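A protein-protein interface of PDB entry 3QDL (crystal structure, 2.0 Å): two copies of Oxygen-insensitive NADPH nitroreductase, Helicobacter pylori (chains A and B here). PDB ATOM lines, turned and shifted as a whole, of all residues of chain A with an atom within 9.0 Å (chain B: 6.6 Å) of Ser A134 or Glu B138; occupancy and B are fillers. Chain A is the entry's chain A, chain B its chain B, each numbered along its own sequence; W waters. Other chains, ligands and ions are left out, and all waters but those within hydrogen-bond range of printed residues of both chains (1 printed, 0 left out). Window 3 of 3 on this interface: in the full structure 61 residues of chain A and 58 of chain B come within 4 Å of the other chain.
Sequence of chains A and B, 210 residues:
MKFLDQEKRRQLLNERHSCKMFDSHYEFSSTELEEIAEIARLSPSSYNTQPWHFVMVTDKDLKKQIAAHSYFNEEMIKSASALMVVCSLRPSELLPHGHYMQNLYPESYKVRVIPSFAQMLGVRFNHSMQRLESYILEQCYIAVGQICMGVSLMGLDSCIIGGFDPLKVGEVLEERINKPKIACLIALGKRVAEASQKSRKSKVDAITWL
The side-chain carboxylate of Glu A138 lies close to the side-chain carboxylate of Glu B138, at 2.5 Å.
The side-chain hydroxyl of Ser A134 sits at hydrogen-bond distance from the backbone carbonyl oxygen of Gln A130, 3.3 Å away.
The backbone carbonyl oxygen (O) of Ala B183 is in hydrogen-bond range of the side-chain hydroxyl (OH) of Tyr B141 (3.3 Å).
Among the printed residues, merely in contact across the chains: Ile A142 with Tyr B141, Tyr A141 with Ile B142, Glu A138 with Tyr B141, Ser A134 with Glu B138, Tyr A141 with Gln B139, Tyr A141 with Glu B138 and Tyr A141 with Tyr B141.
Of chain B, only Glu B138 comes within 4 Å of Ser A134.
Ile A136 touches none of the printed residues of chain B.
Printed residues of chain B within 4 Å of Glu A138: Glu B138 (2.5 Å) and Tyr B141 (3.4 Å).
Printed residues of chain B within 4 Å of Ile A142: Tyr B141 (3.3 Å).
Pro B51 touches none of the printed residues of chain A.
Of the printed residues of chain A, Glu B138 touches Ser A134 (3.5 Å), Glu A138 (2.5 Å) and Tyr A141 (3.6 Å).
Printed residues of chain A within 4 Å of Tyr B141: Glu A138, Tyr A141 and Ile A142.
The nearest residue of chain A that does not touch Glu B138 is Leu A137 (4.5 Å).
Of the 20 printed residues of chain A, 4 touch a printed residue of chain B.
Printed residues of chain A that touch a printed residue of chain B: Ser A134, Glu A138, Tyr A141 and Ile A142.
Hydrophobic or aromatic side chains of chain A within 4 Å of the printed part of chain B: Tyr A141 and Ile A142.
Hydrophobic or aromatic side chains of chain B that line the printed part of chain A: Tyr B141 and Ile B142.
Among the printed residues, 8 pairs touch across the chains.
Among the printed residues, no Asp or Glu carboxylate lies within 4 Å of a Lys or Arg side-chain nitrogen of the other chain.
Glu B138 touches its own counterpart, Glu A138.
Glu A138 touches Tyr B141, and with the chains exchanged Tyr A141 touches Glu B138.
Tyr A141 touches Gln B139, but with the chains exchanged Gln A139 does not touch Tyr B141 (5.5 Å).
Tyr A141 touches Ile B142, and with the chains exchanged Ile A142 touches Tyr B141.
10 positions are printed for both chains.
Of the 8 pairs that touch across the chains among the printed residues, 6 have their exchanged pair printed and touching as well.
Water W1 lies within hydrogen-bond range of the side-chain carboxylate of Glu A138, the side-chain amide nitrogen of Gln A139 and the side-chain hydroxyl of Tyr B141.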
ATOM      1  N   PRO A  51     -16.216  11.023  16.832  1.00  0.00           N
ATOM      2  CA  PRO A  51     -16.253  11.706  15.538  1.00  0.00           C
ATOM      3  C   PRO A  51     -15.773  10.799  14.407  1.00  0.00           C
ATOM      4  O   PRO A  51     -14.879  11.160  13.645  1.00  0.00           O
ATOM      5  CB  PRO A  51     -15.306  12.884  15.747  1.00  0.00           C
ATOM      6  CG  PRO A  51     -14.304  12.383  16.740  1.00  0.00           C
ATOM      7  CD  PRO A  51     -14.965  11.307  17.565  1.00  0.00           C
ATOM      8  N   SER A  88     -13.340  10.103   9.123  1.00  0.00           N
ATOM      9  CA  SER A  88     -13.413  11.183  10.093  1.00  0.00           C
ATOM     10  C   SER A  88     -14.647  12.035   9.823  1.00  0.00           C
ATOM     11  O   SER A  88     -14.968  12.327   8.667  1.00  0.00           O
ATOM     12  CB  SER A  88     -12.143  12.037  10.044  1.00  0.00           C
ATOM     13  OG  SER A  88     -11.726  12.261   8.706  1.00  0.00           O
ATOM     14  N   LEU A  89     -15.347  12.405  10.894  1.00  0.00           N
ATOM     15  CA  LEU A  89     -16.496  13.303  10.818  1.00  0.00           C
ATOM     16  C   LEU A  89     -16.096  14.704  10.364  1.00  0.00           C
ATOM     17  O   LEU A  89     -14.960  15.133  10.576  1.00  0.00           O
ATOM     18  CB  LEU A  89     -17.180  13.403  12.186  1.00  0.00           C
ATOM     19  CG  LEU A  89     -18.626  12.936  12.365  1.00  0.00           C
ATOM     20  CD1 LEU A  89     -18.722  11.428  12.552  1.00  0.00           C
ATOM     21  CD2 LEU A  89     -19.243  13.651  13.554  1.00  0.00           C
ATOM     22  N   PRO A  91     -16.229  18.719  10.910  1.00  0.00           N
ATOM     23  CA  PRO A  91     -16.310  19.562  12.108  1.00  0.00           C
ATOM     24  C   PRO A  91     -17.703  20.168  12.340  1.00  0.00           C
ATOM     25  O   PRO A  91     -18.065  20.453  13.484  1.00  0.00           O
ATOM     26  CB  PRO A  91     -15.287  20.666  11.828  1.00  0.00           C
ATOM     27  CG  PRO A  91     -14.321  20.046  10.874  1.00  0.00           C
ATOM     28  CD  PRO A  91     -15.161  19.169   9.998  1.00  0.00           C
ATOM     29  N   LEU A  94     -19.409  17.577  14.187  1.00  0.00           N
ATOM     30  CA  LEU A  94     -18.802  17.436  15.509  1.00  0.00           C
ATOM     31  C   LEU A  94     -19.494  18.383  16.489  1.00  0.00           C
ATOM     32  O   LEU A  94     -20.018  17.958  17.518  1.00  0.00           O
ATOM     33  CB  LEU A  94     -17.295  17.721  15.450  1.00  0.00           C
ATOM     34  CG  LEU A  94     -16.494  17.635  16.756  1.00  0.00           C
ATOM     35  CD1 LEU A  94     -16.262  16.186  17.166  1.00  0.00           C
ATOM     36  CD2 LEU A  94     -15.170  18.378  16.637  1.00  0.00           C
ATOM     37  N   MET A 129      -3.386  19.553  10.324  1.00  0.00           N
ATOM     38  CA  MET A 129      -2.878  20.860  10.738  1.00  0.00           C
ATOM     39  C   MET A 129      -4.002  21.730  11.312  1.00  0.00           C
ATOM     40  O   MET A 129      -3.773  22.559  12.201  1.00  0.00           O
ATOM     41  CB  MET A 129      -2.186  21.563   9.563  1.00  0.00           C
ATOM     42  CG  MET A 129      -1.148  22.605   9.977  1.00  0.00           C
ATOM     43  SD  MET A 129      -0.444  23.572   8.618  1.00  0.00           S
ATOM     44  CE  MET A 129       0.794  22.447   7.969  1.00  0.00           C
ATOM     45  N   GLN A 130      -5.216  21.533  10.799  1.00  0.00           N
ATOM     46  CA  GLN A 130      -6.391  22.237  11.294  1.00  0.00           C
ATOM     47  C   GLN A 130      -6.748  21.667  12.664  1.00  0.00           C
ATOM     48  O   GLN A 130      -6.846  20.449  12.828  1.00  0.00           O
ATOM     49  CB  GLN A 130      -7.560  22.056  10.330  1.00  0.00           C
ATOM     50  CG  GLN A 130      -8.232  23.348   9.898  1.00  0.00           C
ATOM     51  CD  GLN A 130      -7.564  23.964   8.682  1.00  0.00           C
ATOM     52  OE1 GLN A 130      -7.405  23.310   7.650  1.00  0.00           O
ATOM     53  NE2 GLN A 130      -7.171  25.226   8.799  1.00  0.00           N
ATOM     54  N   ARG A 131      -6.928  22.551  13.642  1.00  0.00           N
ATOM     55  CA  ARG A 131      -7.078  22.138  15.039  1.00  0.00           C
ATOM     56  C   ARG A 131      -8.214  21.137  15.276  1.00  0.00           C
ATOM     57  O   ARG A 131      -7.987  20.091  15.886  1.00  0.00           O
ATOM     58  CB  ARG A 131      -7.180  23.351  15.977  1.00  0.00           C
ATOM     59  CG  ARG A 131      -5.878  24.160  16.112  1.00  0.00           C
ATOM     60  CD  ARG A 131      -4.723  23.310  16.652  1.00  0.00           C
ATOM     61  NE  ARG A 131      -3.498  24.085  16.846  1.00  0.00           N
ATOM     62  CZ  ARG A 131      -2.451  24.068  16.023  1.00  0.00           C
ATOM     63  NH1 ARG A 131      -2.459  23.309  14.935  1.00  0.00           N
ATOM     64  NH2 ARG A 131      -1.388  24.809  16.293  1.00  0.00           N
ATOM     65  N   LEU A 132      -9.411  21.435  14.772  1.00  0.00           N
ATOM     66  CA  LEU A 132     -10.546  20.510  14.912  1.00  0.00           C
ATOM     67  C   LEU A 132     -10.363  19.209  14.135  1.00  0.00           C
ATOM     68  O   LEU A 132     -10.800  18.142  14.577  1.00  0.00           O
ATOM     69  CB  LEU A 132     -11.868  21.171  14.506  1.00  0.00           C
ATOM     70  CG  LEU A 132     -12.616  22.035  15.525  1.00  0.00           C
ATOM     71  CD1 LEU A 132     -14.064  22.209  15.074  1.00  0.00           C
ATOM     72  CD2 LEU A 132     -12.572  21.464  16.936  1.00  0.00           C
ATOM     73  N   GLU A 133      -9.721  19.309  12.976  1.00  0.00           N
ATOM     74  CA  GLU A 133      -9.453  18.150  12.134  1.00  0.00           C
ATOM     75  C   GLU A 133      -8.463  17.191  12.803  1.00  0.00           C
ATOM     76  O   GLU A 133      -8.660  15.973  12.775  1.00  0.00           O
ATOM     77  CB  GLU A 133      -8.955  18.596  10.755  1.00  0.00           C
ATOM     78  CG  GLU A 133     -10.062  19.085   9.801  1.00  0.00           C
ATOM     79  CD  GLU A 133     -10.473  20.548   9.996  1.00  0.00           C
ATOM     80  OE1 GLU A 133     -10.504  21.044  11.147  1.00  0.00           O
ATOM     81  OE2 GLU A 133     -10.785  21.212   8.981  1.00  0.00           O
ATOM     82  N   SER A 134      -7.418  17.747  13.417  1.00  0.00           N
ATOM     83  CA  SER A 134      -6.423  16.946  14.141  1.00  0.00           C
ATOM     84  C   SER A 134      -7.012  16.280  15.388  1.00  0.00           C
ATOM     85  O   SER A 134      -6.706  15.123  15.680  1.00  0.00           O
ATOM     86  CB  SER A 134      -5.211  17.799  14.519  1.00  0.00           C
ATOM     87  OG  SER A 134      -4.464  18.160  13.368  1.00  0.00           O
ATOM     88  N   TYR A 135      -7.852  17.020  16.111  1.00  0.00           N
ATOM     89  CA  TYR A 135      -8.593  16.495  17.260  1.00  0.00           C
ATOM     90  C   TYR A 135      -9.443  15.278  16.881  1.00  0.00           C
ATOM     91  O   TYR A 135      -9.426  14.260  17.574  1.00  0.00           O
ATOM     92  CB  TYR A 135      -9.478  17.594  17.869  1.00  0.00           C
ATOM     93  CG  TYR A 135     -10.498  17.103  18.883  1.00  0.00           C
ATOM     94  CD1 TYR A 135     -10.111  16.742  20.175  1.00  0.00           C
ATOM     95  CD2 TYR A 135     -11.849  17.007  18.549  1.00  0.00           C
ATOM     96  CE1 TYR A 135     -11.044  16.293  21.104  1.00  0.00           C
ATOM     97  CE2 TYR A 135     -12.789  16.560  19.469  1.00  0.00           C
ATOM     98  CZ  TYR A 135     -12.380  16.206  20.744  1.00  0.00           C
ATOM     99  OH  TYR A 135     -13.310  15.766  21.656  1.00  0.00           O
ATOM    100  N   ILE A 136     -10.191  15.403  15.786  1.00  0.00           N
ATOM    101  CA  ILE A 136     -11.063  14.334  15.297  1.00  0.00           C
ATOM    102  C   ILE A 136     -10.262  13.080  14.907  1.00  0.00           C
ATOM    103  O   ILE A 136     -10.667  11.952  15.209  1.00  0.00           O
ATOM    104  CB  ILE A 136     -11.953  14.831  14.122  1.00  0.00           C
ATOM    105  CG1 ILE A 136     -13.094  15.710  14.659  1.00  0.00           C
ATOM    106  CG2 ILE A 136     -12.513  13.660  13.325  1.00  0.00           C
ATOM    107  CD1 ILE A 136     -13.817  16.538  13.589  1.00  0.00           C
ATOM    108  N   LEU A 137      -9.121  13.288  14.253  1.00  0.00           N
ATOM    109  CA  LEU A 137      -8.235  12.188  13.872  1.00  0.00           C
ATOM    110  C   LEU A 137      -7.659  11.451  15.091  1.00  0.00           C
ATOM    111  O   LEU A 137      -7.470  10.231  15.054  1.00  0.00           O
ATOM    112  CB  LEU A 137      -7.110  12.697  12.959  1.00  0.00           C
ATOM    113  CG  LEU A 137      -5.962  11.744  12.590  1.00  0.00           C
ATOM    114  CD1 LEU A 137      -6.438  10.549  11.770  1.00  0.00           C
ATOM    115  CD2 LEU A 137      -4.845  12.490  11.869  1.00  0.00           C
ATOM    116  N   GLU A 138      -7.388  12.200  16.162  1.00  0.00           N
ATOM    117  CA  GLU A 138      -6.873  11.630  17.410  1.00  0.00           C
ATOM    118  C   GLU A 138      -7.849  10.605  17.986  1.00  0.00           C
ATOM    119  O   GLU A 138      -7.437   9.534  18.430  1.00  0.00           O
ATOM    120  CB  GLU A 138      -6.594  12.731  18.436  1.00  0.00           C
ATOM    121  CG  GLU A 138      -5.300  13.487  18.188  1.00  0.00           C
ATOM    122  CD  GLU A 138      -5.086  14.687  19.107  1.00  0.00           C
ATOM    123  OE1 GLU A 138      -5.942  14.979  19.971  1.00  0.00           O
ATOM    124  OE2 GLU A 138      -4.042  15.355  18.957  1.00  0.00           O
ATOM    125  N   GLN A 139      -9.138  10.944  17.964  1.00  0.00           N
ATOM    126  CA  GLN A 139     -10.196  10.059  18.456  1.00  0.00           C
ATOM    127  C   GLN A 139     -10.322   8.827  17.565  1.00  0.00           C
ATOM    128  O   GLN A 139     -10.452   7.708  18.058  1.00  0.00           O
ATOM    129  CB  GLN A 139     -11.540  10.796  18.520  1.00  0.00           C
ATOM    130  CG  GLN A 139     -11.482  12.221  19.084  1.00  0.00           C
ATOM    131  CD  GLN A 139     -10.776  12.296  20.427  1.00  0.00           C
ATOM    132  OE1 GLN A 139     -11.049  11.502  21.326  1.00  0.00           O
ATOM    133  NE2 GLN A 139      -9.859  13.251  20.565  1.00  0.00           N
ATOM    134  N   CYS A 140     -10.278   9.054  16.254  1.00  0.00           N
ATOM    135  CA  CYS A 140     -10.317   7.991  15.254  1.00  0.00           C
ATOM    136  C   CYS A 140      -9.159   7.006  15.423  1.00  0.00           C
ATOM    137  O   CYS A 140      -9.348   5.787  15.325  1.00  0.00           O
ATOM    138  CB  CYS A 140     -10.294   8.595  13.851  1.00  0.00           C
ATOM    139  SG  CYS A 140     -11.900   9.182  13.265  1.00  0.00           S
ATOM    140  N   TYR A 141      -7.968   7.540  15.678  1.00  0.00           N
ATOM    141  CA  TYR A 141      -6.787   6.709  15.913  1.00  0.00           C
ATOM    142  C   TYR A 141      -6.910   5.820  17.156  1.00  0.00           C
ATOM    143  O   TYR A 141      -6.461   4.674  17.142  1.00  0.00           O
ATOM    144  CB  TYR A 141      -5.522   7.565  15.991  1.00  0.00           C
ATOM    145  CG  TYR A 141      -4.858   7.846  14.653  1.00  0.00           C
ATOM    146  CD1 TYR A 141      -5.075   7.021  13.542  1.00  0.00           C
ATOM    147  CD2 TYR A 141      -3.989   8.921  14.508  1.00  0.00           C
ATOM    148  CE1 TYR A 141      -4.445   7.279  12.318  1.00  0.00           C
ATOM    149  CE2 TYR A 141      -3.359   9.186  13.296  1.00  0.00           C
ATOM    150  CZ  TYR A 141      -3.588   8.368  12.210  1.00  0.00           C
ATOM    151  OH  TYR A 141      -2.950   8.648  11.019  1.00  0.00           O
ATOM    152  N   ILE A 142      -7.517   6.348  18.221  1.00  0.00           N
ATOM    153  CA  ILE A 142      -7.811   5.540  19.413  1.00  0.00           C
ATOM    154  C   ILE A 142      -8.653   4.326  19.014  1.00  0.00           C
ATOM    155  O   ILE A 142      -8.284   3.179  19.289  1.00  0.00           O
ATOM    156  CB  ILE A 142      -8.522   6.360  20.523  1.00  0.00           C
ATOM    157  CG1 ILE A 142      -7.561   7.400  21.116  1.00  0.00           C
ATOM    158  CG2 ILE A 142      -9.050   5.437  21.633  1.00  0.00           C
ATOM    159  CD1 ILE A 142      -8.238   8.462  21.958  1.00  0.00           C
ATOM    160  N   LYS A 181     -13.927  12.174   4.503  1.00  0.00           N
ATOM    161  CA  LYS A 181     -12.524  12.376   4.820  1.00  0.00           C
ATOM    162  C   LYS A 181     -12.025  11.090   5.475  1.00  0.00           C
ATOM    163  O   LYS A 181     -12.542  10.665   6.513  1.00  0.00           O
ATOM    164  CB  LYS A 181     -12.333  13.592   5.731  1.00  0.00           C
ATOM    165  CG  LYS A 181     -10.882  14.051   5.861  1.00  0.00           C
ATOM    166  CD  LYS A 181     -10.785  15.436   6.491  1.00  0.00           C
ATOM    167  CE  LYS A 181      -9.340  15.916   6.589  1.00  0.00           C
ATOM    168  NZ  LYS A 181      -8.683  16.081   5.254  1.00  0.00           N
ATOM    169  N   PRO B  51       6.309   6.984  16.678  1.00  0.00           N
ATOM    170  CA  PRO B  51       6.508   8.411  16.941  1.00  0.00           C
ATOM    171  C   PRO B  51       6.054   8.812  18.344  1.00  0.00           C
ATOM    172  O   PRO B  51       5.242   9.730  18.496  1.00  0.00           O
ATOM    173  CB  PRO B  51       5.622   9.072  15.883  1.00  0.00           C
ATOM    174  CG  PRO B  51       4.491   8.124  15.726  1.00  0.00           C
ATOM    175  CD  PRO B  51       5.066   6.741  15.917  1.00  0.00           C
ATOM    176  N   SER B  88       4.458  12.629  22.257  1.00  0.00           N
ATOM    177  CA  SER B  88       4.824  12.487  20.848  1.00  0.00           C
ATOM    178  C   SER B  88       6.180  13.136  20.572  1.00  0.00           C
ATOM    179  O   SER B  88       6.489  14.196  21.117  1.00  0.00           O
ATOM    180  CB  SER B  88       3.756  13.108  19.947  1.00  0.00           C
ATOM    181  OG  SER B  88       3.816  14.524  19.981  1.00  0.00           O
ATOM    182  N   TYR B 135      -1.155  12.982   9.547  1.00  0.00           N
ATOM    183  CA  TYR B 135       0.077  13.220  10.298  1.00  0.00           C
ATOM    184  C   TYR B 135       0.457  12.178  11.350  1.00  0.00           C
ATOM    185  O   TYR B 135      -0.374  11.699  12.128  1.00  0.00           O
ATOM    186  CB  TYR B 135       0.155  14.661  10.817  1.00  0.00           C
ATOM    187  CG  TYR B 135       0.882  15.545   9.829  1.00  0.00           C
ATOM    188  CD1 TYR B 135       2.196  15.947  10.062  1.00  0.00           C
ATOM    189  CD2 TYR B 135       0.277  15.928   8.629  1.00  0.00           C
ATOM    190  CE1 TYR B 135       2.878  16.739   9.141  1.00  0.00           C
ATOM    191  CE2 TYR B 135       0.948  16.714   7.703  1.00  0.00           C
ATOM    192  CZ  TYR B 135       2.246  17.118   7.962  1.00  0.00           C
ATOM    193  OH  TYR B 135       2.909  17.901   7.043  1.00  0.00           O
ATOM    194  N   ILE B 136       1.744  11.847  11.332  1.00  0.00           N
ATOM    195  CA  ILE B 136       2.320  10.729  12.071  1.00  0.00           C
ATOM    196  C   ILE B 136       2.429  11.022  13.566  1.00  0.00           C
ATOM    197  O   ILE B 136       2.357  10.108  14.389  1.00  0.00           O
ATOM    198  CB  ILE B 136       3.706  10.345  11.471  1.00  0.00           C
ATOM    199  CG1 ILE B 136       3.560  10.004   9.981  1.00  0.00           C
ATOM    200  CG2 ILE B 136       4.333   9.167  12.219  1.00  0.00           C
ATOM    201  CD1 ILE B 136       4.801  10.279   9.145  1.00  0.00           C
ATOM    202  N   LEU B 137       2.567  12.298  13.918  1.00  0.00           N
ATOM    203  CA  LEU B 137       2.748  12.683  15.319  1.00  0.00           C
ATOM    204  C   LEU B 137       1.480  12.546  16.168  1.00  0.00           C
ATOM    205  O   LEU B 137       1.513  12.771  17.379  1.00  0.00           O
ATOM    206  CB  LEU B 137       3.355  14.091  15.436  1.00  0.00           C
ATOM    207  CG  LEU B 137       4.803  14.277  14.958  1.00  0.00           C
ATOM    208  CD1 LEU B 137       5.230  15.736  15.094  1.00  0.00           C
ATOM    209  CD2 LEU B 137       5.793  13.358  15.691  1.00  0.00           C
ATOM    210  N   GLU B 138       0.374  12.163  15.531  1.00  0.00           N
ATOM    211  CA  GLU B 138      -0.877  11.891  16.239  1.00  0.00           C
ATOM    212  C   GLU B 138      -1.036  10.404  16.562  1.00  0.00           C
ATOM    213  O   GLU B 138      -1.977  10.010  17.255  1.00  0.00           O
ATOM    214  CB  GLU B 138      -2.082  12.382  15.426  1.00  0.00           C
ATOM    215  CG  GLU B 138      -2.133  13.896  15.177  1.00  0.00           C
ATOM    216  CD  GLU B 138      -2.435  14.715  16.425  1.00  0.00           C
ATOM    217  OE1 GLU B 138      -2.254  14.212  17.552  1.00  0.00           O
ATOM    218  OE2 GLU B 138      -2.852  15.880  16.280  1.00  0.00           O
ATOM    219  N   GLN B 139      -0.107   9.586  16.074  1.00  0.00           N
ATOM    220  CA  GLN B 139      -0.254   8.131  16.142  1.00  0.00           C
ATOM    221  C   GLN B 139       0.051   7.507  17.502  1.00  0.00           C
ATOM    222  O   GLN B 139      -0.084   6.291  17.670  1.00  0.00           O
ATOM    223  CB  GLN B 139       0.546   7.455  15.028  1.00  0.00           C
ATOM    224  CG  GLN B 139      -0.015   7.753  13.647  1.00  0.00           C
ATOM    225  CD  GLN B 139       0.750   7.082  12.527  1.00  0.00           C
ATOM    226  OE1 GLN B 139       1.644   6.261  12.760  1.00  0.00           O
ATOM    227  NE2 GLN B 139       0.394   7.424  11.293  1.00  0.00           N
ATOM    228  N   CYS B 140       0.438   8.340  18.471  1.00  0.00           N
ATOM    229  CA  CYS B 140       0.504   7.926  19.875  1.00  0.00           C
ATOM    230  C   CYS B 140      -0.891   7.555  20.382  1.00  0.00           C
ATOM    231  O   CYS B 140      -1.036   6.778  21.323  1.00  0.00           O
ATOM    232  CB  CYS B 140       1.130   9.020  20.757  1.00  0.00           C
ATOM    233  SG  CYS B 140       0.294  10.645  20.741  1.00  0.00           S
ATOM    234  N   TYR B 141      -1.915   8.105  19.732  1.00  0.00           N
ATOM    235  CA  TYR B 141      -3.299   7.780  20.053  1.00  0.00           C
ATOM    236  C   TYR B 141      -3.712   6.369  19.615  1.00  0.00           C
ATOM    237  O   TYR B 141      -4.614   5.783  20.210  1.00  0.00           O
ATOM    238  CB  TYR B 141      -4.243   8.863  19.520  1.00  0.00           C
ATOM    239  CG  TYR B 141      -4.104  10.154  20.296  1.00  0.00           C
ATOM    240  CD1 TYR B 141      -4.900  10.404  21.413  1.00  0.00           C
ATOM    241  CD2 TYR B 141      -3.148  11.109  19.940  1.00  0.00           C
ATOM    242  CE1 TYR B 141      -4.767  11.581  22.141  1.00  0.00           C
ATOM    243  CE2 TYR B 141      -3.003  12.288  20.665  1.00  0.00           C
ATOM    244  CZ  TYR B 141      -3.819  12.514  21.763  1.00  0.00           C
ATOM    245  OH  TYR B 141      -3.685  13.672  22.489  1.00  0.00           O
ATOM    246  N   ILE B 142      -3.045   5.821  18.600  1.00  0.00           N
ATOM    247  CA  ILE B 142      -3.233   4.406  18.243  1.00  0.00           C
ATOM    248  C   ILE B 142      -2.755   3.517  19.393  1.00  0.00           C
ATOM    249  O   ILE B 142      -3.383   2.504  19.707  1.00  0.00           O
ATOM    250  CB  ILE B 142      -2.522   4.016  16.917  1.00  0.00           C
ATOM    251  CG1 ILE B 142      -3.265   4.617  15.718  1.00  0.00           C
ATOM    252  CG2 ILE B 142      -2.450   2.491  16.754  1.00  0.00           C
ATOM    253  CD1 ILE B 142      -2.466   4.605  14.426  1.00  0.00           C
ATOM    254  N   ALA B 183       0.828  14.552  24.944  1.00  0.00           N
ATOM    255  CA  ALA B 183      -0.415  14.399  24.196  1.00  0.00           C
ATOM    256  C   ALA B 183      -1.604  14.287  25.145  1.00  0.00           C
ATOM    257  O   ALA B 183      -2.494  15.140  25.141  1.00  0.00           O
ATOM    258  CB  ALA B 183      -0.337  13.187  23.282  1.00  0.00           C
HETATM  259  O   HOH W   1      -7.079  14.017  22.006  1.00  0.00           O
